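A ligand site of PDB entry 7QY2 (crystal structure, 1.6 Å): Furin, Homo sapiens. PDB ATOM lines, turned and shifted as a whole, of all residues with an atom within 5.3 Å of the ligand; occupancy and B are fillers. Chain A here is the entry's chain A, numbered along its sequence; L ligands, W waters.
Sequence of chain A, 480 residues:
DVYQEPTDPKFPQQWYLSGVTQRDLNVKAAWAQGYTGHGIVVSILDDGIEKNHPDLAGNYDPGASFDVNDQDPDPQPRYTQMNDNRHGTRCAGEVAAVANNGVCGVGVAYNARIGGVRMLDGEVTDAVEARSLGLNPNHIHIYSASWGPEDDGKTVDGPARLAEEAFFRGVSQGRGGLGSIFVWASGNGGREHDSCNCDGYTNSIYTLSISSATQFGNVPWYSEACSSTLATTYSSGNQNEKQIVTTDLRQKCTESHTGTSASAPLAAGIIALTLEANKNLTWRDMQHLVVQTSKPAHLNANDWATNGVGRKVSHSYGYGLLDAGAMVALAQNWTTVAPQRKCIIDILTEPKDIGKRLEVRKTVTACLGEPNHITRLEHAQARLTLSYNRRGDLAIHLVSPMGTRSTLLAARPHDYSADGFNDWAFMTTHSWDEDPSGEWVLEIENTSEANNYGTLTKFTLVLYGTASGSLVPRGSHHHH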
ATOM      1  N   LEU A  45      10.055  26.162   0.113  1.00  0.00           N
ATOM      2  CA  LEU A  45      10.695  26.624   1.353  1.00  0.00           C
ATOM      3  C   LEU A  45      11.341  27.974   1.068  1.00  0.00           C
ATOM      4  O   LEU A  45      12.398  28.055   0.432  1.00  0.00           O
ATOM      5  CB  LEU A  45      11.712  25.602   1.848  1.00  0.00           C
ATOM      6  CG  LEU A  45      11.159  24.498   2.750  1.00  0.00           C
ATOM      7  CD1 LEU A  45      10.044  23.725   2.060  1.00  0.00           C
ATOM      8  CD2 LEU A  45      12.263  23.532   3.180  1.00  0.00           C
ATOM      9  N   ASP A  46      10.704  29.061   1.520  1.00  0.00           N
ATOM     10  CA  ASP A  46      11.144  30.397   1.123  1.00  0.00           C
ATOM     11  C   ASP A  46      10.560  31.489   2.015  1.00  0.00           C
ATOM     12  O   ASP A  46      10.487  31.313   3.237  1.00  0.00           O
ATOM     13  CB  ASP A  46      10.757  30.588  -0.356  1.00  0.00           C
ATOM     14  CG  ASP A  46      11.710  31.502  -1.105  1.00  0.00           C
ATOM     15  OD1 ASP A  46      11.879  32.669  -0.704  1.00  0.00           O
ATOM     16  OD2 ASP A  46      12.278  31.052  -2.134  1.00  0.00           O
ATOM     17  N   ASP A  47      10.195  32.630   1.426  1.00  0.00           N
ATOM     18  CA  ASP A  47       9.767  33.786   2.209  1.00  0.00           C
ATOM     19  C   ASP A  47       8.253  33.904   2.300  1.00  0.00           C
ATOM     20  O   ASP A  47       7.752  34.971   2.707  1.00  0.00           O
ATOM     21  CB  ASP A  47      10.356  35.068   1.606  1.00  0.00           C
ATOM     22  CG  ASP A  47       9.997  35.245   0.136  1.00  0.00           C
ATOM     23  OD1 ASP A  47       9.040  34.594  -0.335  1.00  0.00           O
ATOM     24  OD2 ASP A  47      10.687  36.039  -0.540  1.00  0.00           O
ATOM     25  N   ASP A  84       9.767  42.756  -0.866  1.00  0.00           N
ATOM     26  CA  ASP A  84      10.876  41.911  -0.437  1.00  0.00           C
ATOM     27  C   ASP A  84      10.546  40.431  -0.474  1.00  0.00           C
ATOM     28  O   ASP A  84      11.410  39.601  -0.769  1.00  0.00           O
ATOM     29  CB  ASP A  84      11.255  42.273   0.999  1.00  0.00           C
ATOM     30  CG  ASP A  84      11.865  43.629   1.118  1.00  0.00           C
ATOM     31  OD1 ASP A  84      13.087  43.710   0.920  1.00  0.00           O
ATOM     32  OD2 ASP A  84      11.128  44.595   1.416  1.00  0.00           O
ATOM     33  N   ARG A  86       8.602  38.321  -2.121  1.00  0.00           N
ATOM     34  CA  ARG A  86       7.890  37.853  -3.302  1.00  0.00           C
ATOM     35  C   ARG A  86       8.444  36.549  -3.857  1.00  0.00           C
ATOM     36  O   ARG A  86       7.818  35.977  -4.754  1.00  0.00           O
ATOM     37  CB  ARG A  86       7.949  38.917  -4.399  1.00  0.00           C
ATOM     38  CG  ARG A  86       9.348  39.097  -4.968  1.00  0.00           C
ATOM     39  CD  ARG A  86       9.379  40.273  -5.915  1.00  0.00           C
ATOM     40  NE  ARG A  86      10.687  40.369  -6.562  1.00  0.00           N
ATOM     41  CZ  ARG A  86      11.071  41.379  -7.337  1.00  0.00           C
ATOM     42  NH1 ARG A  86      10.246  42.394  -7.572  1.00  0.00           N
ATOM     43  NH2 ARG A  86      12.285  41.366  -7.873  1.00  0.00           N
ATOM     44  N   HIS A  87       9.593  36.081  -3.373  1.00  0.00           N
ATOM     45  CA  HIS A  87      10.271  35.016  -4.101  1.00  0.00           C
ATOM     46  C   HIS A  87       9.523  33.699  -4.008  1.00  0.00           C
ATOM     47  O   HIS A  87       9.425  32.958  -4.994  1.00  0.00           O
ATOM     48  CB  HIS A  87      11.712  34.853  -3.602  1.00  0.00           C
ATOM     49  CG  HIS A  87      12.542  34.049  -4.538  1.00  0.00           C
ATOM     50  ND1 HIS A  87      12.763  32.696  -4.369  1.00  0.00           N
ATOM     51  CD2 HIS A  87      13.171  34.383  -5.692  1.00  0.00           C
ATOM     52  CE1 HIS A  87      13.513  32.252  -5.365  1.00  0.00           C
ATOM     53  NE2 HIS A  87      13.770  33.243  -6.180  1.00  0.00           N
ATOM     54  N   MET A 119       9.784  30.723   5.969  1.00  0.00           N
ATOM     55  CA  MET A 119      10.922  30.460   6.853  1.00  0.00           C
ATOM     56  C   MET A 119      12.061  31.455   6.715  1.00  0.00           C
ATOM     57  O   MET A 119      12.866  31.564   7.656  1.00  0.00           O
ATOM     58  CB  MET A 119      11.491  29.049   6.611  1.00  0.00           C
ATOM     59  CG  MET A 119      12.060  28.841   5.210  1.00  0.00           C
ATOM     60  SD  MET A 119      12.798  27.215   4.961  1.00  0.00           S
ATOM     61  CE  MET A 119      14.102  27.318   6.174  1.00  0.00           C
ATOM     62  N   LEU A 120      12.180  32.169   5.612  1.00  0.00           N
ATOM     63  CA  LEU A 120      13.314  33.054   5.368  1.00  0.00           C
ATOM     64  C   LEU A 120      13.059  34.495   5.788  1.00  0.00           C
ATOM     65  O   LEU A 120      13.960  35.322   5.649  1.00  0.00           O
ATOM     66  CB  LEU A 120      13.727  33.029   3.895  1.00  0.00           C
ATOM     67  CG  LEU A 120      14.077  31.643   3.324  1.00  0.00           C
ATOM     68  CD1 LEU A 120      14.487  31.735   1.857  1.00  0.00           C
ATOM     69  CD2 LEU A 120      15.170  30.973   4.152  1.00  0.00           C
ATOM     70  N   VAL A 124      17.136  32.604  10.487  1.00  0.00           N
ATOM     71  CA  VAL A 124      17.109  31.215  10.044  1.00  0.00           C
ATOM     72  C   VAL A 124      18.051  30.441  10.968  1.00  0.00           C
ATOM     73  O   VAL A 124      19.277  30.490  10.821  1.00  0.00           O
ATOM     74  CB  VAL A 124      17.494  31.065   8.574  1.00  0.00           C
ATOM     75  CG1 VAL A 124      17.486  29.590   8.174  1.00  0.00           C
ATOM     76  CG2 VAL A 124      16.526  31.855   7.707  1.00  0.00           C
ATOM     77  N   THR A 125      17.470  29.724  11.913  1.00  0.00           N
ATOM     78  CA  THR A 125      18.176  28.881  12.855  1.00  0.00           C
ATOM     79  C   THR A 125      18.082  27.416  12.411  1.00  0.00           C
ATOM     80  O   THR A 125      17.300  27.052  11.548  1.00  0.00           O
ATOM     81  CB  THR A 125      17.567  29.003  14.249  1.00  0.00           C
ATOM     82  OG1 THR A 125      16.204  28.553  14.192  1.00  0.00           O
ATOM     83  CG2 THR A 125      17.603  30.444  14.743  1.00  0.00           C
ATOM     84  N   ASP A 126      18.887  26.568  13.067  1.00  0.00           N
ATOM     85  CA  ASP A 126      18.813  25.136  12.850  1.00  0.00           C
ATOM     86  C   ASP A 126      17.402  24.603  13.094  1.00  0.00           C
ATOM     87  O   ASP A 126      16.874  23.817  12.298  1.00  0.00           O
ATOM     88  CB  ASP A 126      19.845  24.466  13.768  1.00  0.00           C
ATOM     89  CG  ASP A 126      19.947  22.968  13.575  1.00  0.00           C
ATOM     90  OD1 ASP A 126      19.837  22.487  12.433  1.00  0.00           O
ATOM     91  OD2 ASP A 126      20.188  22.286  14.593  1.00  0.00           O
ATOM     92  N   GLU A 129      15.075  25.599  10.232  1.00  0.00           N
ATOM     93  CA  GLU A 129      15.332  24.730   9.095  1.00  0.00           C
ATOM     94  C   GLU A 129      14.720  23.345   9.291  1.00  0.00           C
ATOM     95  O   GLU A 129      14.097  22.795   8.375  1.00  0.00           O
ATOM     96  CB  GLU A 129      16.840  24.610   8.869  1.00  0.00           C
ATOM     97  CG  GLU A 129      17.515  25.921   8.487  1.00  0.00           C
ATOM     98  CD  GLU A 129      19.018  25.783   8.293  1.00  0.00           C
ATOM     99  OE1 GLU A 129      19.496  24.635   8.171  1.00  0.00           O
ATOM    100  OE2 GLU A 129      19.714  26.813   8.274  1.00  0.00           O
ATOM    101  N   LEU A 133      11.988  21.589   6.786  1.00  0.00           N
ATOM    102  CA  LEU A 133      12.250  20.364   6.053  1.00  0.00           C
ATOM    103  C   LEU A 133      11.357  19.231   6.512  1.00  0.00           C
ATOM    104  O   LEU A 133      11.007  18.356   5.715  1.00  0.00           O
ATOM    105  CB  LEU A 133      13.716  19.971   6.233  1.00  0.00           C
ATOM    106  CG  LEU A 133      14.747  20.931   5.625  1.00  0.00           C
ATOM    107  CD1 LEU A 133      16.106  20.645   6.240  1.00  0.00           C
ATOM    108  CD2 LEU A 133      14.787  20.787   4.133  1.00  0.00           C
ATOM    109  N   ALA A 145      13.805  24.102  -2.405  1.00  0.00           N
ATOM    110  CA  ALA A 145      14.565  25.116  -1.682  1.00  0.00           C
ATOM    111  C   ALA A 145      15.585  25.767  -2.608  1.00  0.00           C
ATOM    112  O   ALA A 145      16.417  25.077  -3.203  1.00  0.00           O
ATOM    113  CB  ALA A 145      15.286  24.503  -0.471  1.00  0.00           C
ATOM    114  N   SER A 146      15.528  27.088  -2.703  1.00  0.00           N
ATOM    115  CA  SER A 146      16.329  27.816  -3.680  1.00  0.00           C
ATOM    116  C   SER A 146      17.535  28.513  -3.064  1.00  0.00           C
ATOM    117  O   SER A 146      18.284  29.179  -3.783  1.00  0.00           O
ATOM    118  CB  SER A 146      15.442  28.842  -4.390  1.00  0.00           C
ATOM    119  OG  SER A 146      14.631  28.181  -5.364  1.00  0.00           O
ATOM    120  N   TRP A 147      17.780  28.327  -1.774  1.00  0.00           N
ATOM    121  CA  TRP A 147      18.763  29.127  -1.061  1.00  0.00           C
ATOM    122  C   TRP A 147      19.477  28.276  -0.019  1.00  0.00           C
ATOM    123  O   TRP A 147      19.082  27.144   0.274  1.00  0.00           O
ATOM    124  CB  TRP A 147      18.098  30.329  -0.379  1.00  0.00           C
ATOM    125  CG  TRP A 147      17.121  31.070  -1.216  1.00  0.00           C
ATOM    126  CD1 TRP A 147      15.752  30.933  -1.225  1.00  0.00           C
ATOM    127  CD2 TRP A 147      17.415  32.108  -2.157  1.00  0.00           C
ATOM    128  NE1 TRP A 147      15.191  31.814  -2.112  1.00  0.00           N
ATOM    129  CE2 TRP A 147      16.192  32.548  -2.704  1.00  0.00           C
ATOM    130  CE3 TRP A 147      18.606  32.700  -2.603  1.00  0.00           C
ATOM    131  CZ2 TRP A 147      16.119  33.549  -3.664  1.00  0.00           C
ATOM    132  CZ3 TRP A 147      18.526  33.698  -3.557  1.00  0.00           C
ATOM    133  CH2 TRP A 147      17.301  34.117  -4.085  1.00  0.00           C
ATOM    134  N   GLY A 148      20.516  28.858   0.558  1.00  0.00           N
ATOM    135  CA  GLY A 148      21.326  28.188   1.542  1.00  0.00           C
ATOM    136  C   GLY A 148      22.284  29.150   2.211  1.00  0.00           C
ATOM    137  O   GLY A 148      21.999  30.347   2.354  1.00  0.00           O
ATOM    138  N   PRO A 149      23.447  28.648   2.645  1.00  0.00           N
ATOM    139  CA  PRO A 149      24.465  29.533   3.202  1.00  0.00           C
ATOM    140  C   PRO A 149      24.851  30.608   2.209  1.00  0.00           C
ATOM    141  O   PRO A 149      24.681  30.462   1.001  1.00  0.00           O
ATOM    142  CB  PRO A 149      25.652  28.611   3.511  1.00  0.00           C
ATOM    143  CG  PRO A 149      25.149  27.248   3.366  1.00  0.00           C
ATOM    144  CD  PRO A 149      23.935  27.262   2.498  1.00  0.00           C
ATOM    145  N   ASP A 157      29.501  25.962   5.017  1.00  0.00           N
ATOM    146  CA  ASP A 157      28.509  25.668   6.035  1.00  0.00           C
ATOM    147  C   ASP A 157      27.446  24.765   5.419  1.00  0.00           C
ATOM    148  O   ASP A 157      27.297  24.685   4.203  1.00  0.00           O
ATOM    149  CB  ASP A 157      27.884  26.944   6.623  1.00  0.00           C
ATOM    150  CG  ASP A 157      27.369  26.759   8.055  1.00  0.00           C
ATOM    151  OD1 ASP A 157      27.506  25.655   8.643  1.00  0.00           O
ATOM    152  OD2 ASP A 157      26.813  27.733   8.607  1.00  0.00           O
ATOM    153  N   GLY A 158      26.710  24.102   6.295  1.00  0.00           N
ATOM    154  CA  GLY A 158      25.679  23.172   5.892  1.00  0.00           C
ATOM    155  C   GLY A 158      24.726  22.954   7.037  1.00  0.00           C
ATOM    156  O   GLY A 158      24.776  23.636   8.067  1.00  0.00           O
ATOM    157  N   PRO A 159      23.832  21.973   6.889  1.00  0.00           N
ATOM    158  CA  PRO A 159      22.843  21.739   7.955  1.00  0.00           C
ATOM    159  C   PRO A 159      23.513  21.376   9.275  1.00  0.00           C
ATOM    160  O   PRO A 159      24.401  20.515   9.339  1.00  0.00           O
ATOM    161  CB  PRO A 159      22.004  20.569   7.399  1.00  0.00           C
ATOM    162  CG  PRO A 159      22.883  19.919   6.356  1.00  0.00           C
ATOM    163  CD  PRO A 159      23.676  21.045   5.764  1.00  0.00           C
ATOM    164  N   ALA A 160      23.087  22.065  10.342  1.00  0.00           N
ATOM    165  CA  ALA A 160      23.474  21.725  11.702  1.00  0.00           C
ATOM    166  C   ALA A 160      22.642  20.506  12.126  1.00  0.00           C
ATOM    167  O   ALA A 160      21.968  19.874  11.303  1.00  0.00           O
ATOM    168  CB  ALA A 160      23.309  22.934  12.617  1.00  0.00           C
ATOM    169  N   TRP A 184      17.058  21.069  -4.559  1.00  0.00           N
ATOM    170  CA  TRP A 184      17.873  22.216  -4.152  1.00  0.00           C
ATOM    171  C   TRP A 184      18.490  22.935  -5.340  1.00  0.00           C
ATOM    172  O   TRP A 184      18.904  22.298  -6.316  1.00  0.00           O
ATOM    173  CB  TRP A 184      19.023  21.806  -3.200  1.00  0.00           C
ATOM    174  CG  TRP A 184      19.098  22.706  -2.021  1.00  0.00           C
ATOM    175  CD1 TRP A 184      19.806  23.870  -1.916  1.00  0.00           C
ATOM    176  CD2 TRP A 184      18.407  22.548  -0.791  1.00  0.00           C
ATOM    177  NE1 TRP A 184      19.588  24.450  -0.683  1.00  0.00           N
ATOM    178  CE2 TRP A 184      18.737  23.652   0.030  1.00  0.00           C
ATOM    179  CE3 TRP A 184      17.536  21.577  -0.292  1.00  0.00           C
ATOM    180  CZ2 TRP A 184      18.228  23.795   1.310  1.00  0.00           C
ATOM    181  CZ3 TRP A 184      17.029  21.731   0.979  1.00  0.00           C
ATOM    182  CH2 TRP A 184      17.372  22.832   1.766  1.00  0.00           C
ATOM    183  N   TYR A 201      23.970  21.926   1.972  1.00  0.00           N
ATOM    184  CA  TYR A 201      22.630  21.552   1.550  1.00  0.00           C
ATOM    185  C   TYR A 201      22.654  20.971   0.147  1.00  0.00           C
ATOM    186  O   TYR A 201      22.195  19.858  -0.081  1.00  0.00           O
ATOM    187  CB  TYR A 201      21.700  22.774   1.627  1.00  0.00           C
ATOM    188  CG  TYR A 201      21.642  23.328   3.027  1.00  0.00           C
ATOM    189  CD1 TYR A 201      22.659  24.144   3.502  1.00  0.00           C
ATOM    190  CD2 TYR A 201      20.607  23.000   3.901  1.00  0.00           C
ATOM    191  CE1 TYR A 201      22.648  24.638   4.784  1.00  0.00           C
ATOM    192  CE2 TYR A 201      20.586  23.495   5.203  1.00  0.00           C
ATOM    193  CZ  TYR A 201      21.623  24.310   5.638  1.00  0.00           C
ATOM    194  OH  TYR A 201      21.642  24.826   6.916  1.00  0.00           O
HETATM  195  C1  LIG L   1      25.408  25.598  14.560  1.00  0.00           C
HETATM  196  C2  LIG L   1      24.047  26.125  14.105  1.00  0.00           C
HETATM  197  C3  LIG L   1      22.789  27.247  12.330  1.00  0.00           C
HETATM  198  C4  LIG L   1      23.020  27.669  10.882  1.00  0.00           C
HETATM  199  C5  LIG L   1      23.249  26.432  10.010  1.00  0.00           C
HETATM  200  C6  LIG L   1      23.455  26.874   8.560  1.00  0.00           C
HETATM  201  C7  LIG L   1      22.031  28.805   8.878  1.00  0.00           C
HETATM  202  C8  LIG L   1      21.809  28.437  10.347  1.00  0.00           C
HETATM  203  C9  LIG L   1      22.524  28.022   6.611  1.00  0.00           C
HETATM  204  C10 LIG L   1      21.383  28.587   5.948  1.00  0.00           C
HETATM  205  C11 LIG L   1      21.265  29.954   5.822  1.00  0.00           C
HETATM  206  C12 LIG L   1      20.154  30.492   5.164  1.00  0.00           C
HETATM  207  C13 LIG L   1      19.269  28.379   4.768  1.00  0.00           C
HETATM  208  C14 LIG L   1      20.373  27.793   5.412  1.00  0.00           C
HETATM  209  C15 LIG L   1      18.208  27.614   4.236  1.00  0.00           C
HETATM  210  C16 LIG L   1      17.859  26.406   4.829  1.00  0.00           C
HETATM  211  C17 LIG L   1      16.789  25.649   4.338  1.00  0.00           C
HETATM  212  C18 LIG L   1      16.055  26.104   3.258  1.00  0.00           C
HETATM  213  C19 LIG L   1      16.382  27.328   2.680  1.00  0.00           C
HETATM  214  C20 LIG L   1      17.441  28.076   3.170  1.00  0.00           C
HETATM  215  C21 LIG L   1      19.266  32.482   4.235  1.00  0.00           C
HETATM  216  C22 LIG L   1      18.486  33.520   4.708  1.00  0.00           C
HETATM  217  C23 LIG L   1      17.651  33.857   2.528  1.00  0.00           C
HETATM  218  C24 LIG L   1      19.256  32.157   2.886  1.00  0.00           C
HETATM  219  C25 LIG L   1      16.137  35.675   2.234  1.00  0.00           C
HETATM  220  C26 LIG L   1      16.219  36.855   1.298  1.00  0.00           C
HETATM  221  C27 LIG L   1      15.806  37.686  -0.868  1.00  0.00           C
HETATM  222  C28 LIG L   1      15.396  37.349  -2.278  1.00  0.00           C
HETATM  223  C29 LIG L   1      15.073  38.627  -3.040  1.00  0.00           C
HETATM  224  C30 LIG L   1      16.270  39.541  -3.230  1.00  0.00           C
HETATM  225  C31 LIG L   1      14.623  38.154  -4.418  1.00  0.00           C
HETATM  226  C32 LIG L   1      17.020  35.604  -0.533  1.00  0.00           C
HETATM  227  C33 LIG L   1      16.983  34.291   0.234  1.00  0.00           C
HETATM  228  N1  LIG L   1      24.038  26.691  12.898  1.00  0.00           N
HETATM  229  N2  LIG L   1      22.283  27.629   8.014  1.00  0.00           N
HETATM  230  N3  LIG L   1      19.187  29.719   4.670  1.00  0.00           N
HETATM  231  N4  LIG L   1      17.673  34.195   3.819  1.00  0.00           N
HETATM  232  N5  LIG L   1      18.424  32.875   2.042  1.00  0.00           N
HETATM  233  N6  LIG L   1      16.907  34.553   1.694  1.00  0.00           N
HETATM  234  N7  LIG L   1      15.919  36.455  -0.083  1.00  0.00           N
HETATM  235  O1  LIG L   1      23.047  26.022  14.810  1.00  0.00           O
HETATM  236  O2  LIG L   1      20.077  31.846   5.095  1.00  0.00           O
HETATM  237  O3  LIG L   1      15.511  38.095  -5.295  1.00  0.00           O
HETATM  238  O4  LIG L   1      13.438  37.782  -4.553  1.00  0.00           O
HETATM  239 CL1  LIG L   1      16.378  24.147   5.113  1.00  0.00          CL
HETATM  240 CL2  LIG L   1      15.431  27.890   1.344  1.00  0.00          CL
HETATM  241  O   HOH W   1      20.832  27.571  15.006  1.00  0.00           O
HETATM  242  O   HOH W   2      13.329  35.055  -0.474  1.00  0.00           O
HETATM  243  O   HOH W   3      15.942  36.761  -7.438  1.00  0.00           O
HETATM  244  O   HOH W   4      25.424  29.705   7.344  1.00  0.00           O
HETATM  245  O   HOH W   5      22.355  33.077   2.639  1.00  0.00           O
HETATM  246  O   HOH W   6      26.484  27.301  11.424  1.00  0.00           O
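Water W1 bridges an oxygen (O1) of the ligand and the backbone NH (N) of Asp 126.
Water W6 bridges the side-chain carboxylate (OD2) of Asp 157 (2.9 Å) and a nitrogen (N1) of the ligand (2.9 Å).
Water W2 lies within hydrogen-bond range of OD1 of Asp 46, OD2 of Asp 47 and N7 of the ligand.
Residues that only touch the ligand: Leu 45, Trp 147, Val 124, Gly 148, Asp 157, His 87, Gly 158, Ala 160, Leu 133, Met 119, Asp 126, Leu 120, Trp 184, Ala 145 and Pro 149.
Hydrophobic or aromatic side chains within 4 Å of the ligand: His 87, Met 119, Leu 120, Val 124, Leu 133, Ala 145, Trp 147, Ala 160, Trp 184 and Tyr 201.
The nearest printed residue that does not touch the ligand is Ser 146 (4.1 Å).
The side-chain hydroxyl of Tyr 201 is in hydrogen-bond range of the side-chain carboxylate of Glu 129.
A ring nitrogen (ND1) of His 87 lies within hydrogen-bond range of the indole nitrogen of Trp 147, 3.4 Å away.
The indole nitrogen (NE1) of Trp 184 sits at hydrogen-bond distance from the backbone carbonyl oxygen (O) of Trp 147 (2.9 Å).
The indole nitrogen of Trp 147 lies within hydrogen-bond range of the side-chain carboxylate of Asp 46, at 3.0 Å.
A ring nitrogen (ND1) of His 87 lies within hydrogen-bond range of the side-chain carboxylate of Asp 46, at 2.8 Å.
The backbone NH (N) of His 87 is in hydrogen-bond range of the side-chain carboxylate (OD2) of Asp 47, 3.0 Å away.
The backbone NH (N) of Met 119 sits at hydrogen-bond distance from the backbone carbonyl oxygen (O) of Asp 46, 2.9 Å away.
The backbone NH (N) of Leu 120 sits at hydrogen-bond distance from the backbone carbonyl oxygen (O) of Asp 46 (3.0 Å).
OE2 of Glu 129 lies within salt-bridge range of N2 of the ligand (2.7 Å).
The side-chain hydroxyl of Tyr 201 sits at hydrogen-bond distance from a nitrogen (N2) of the ligand (3.1 Å).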
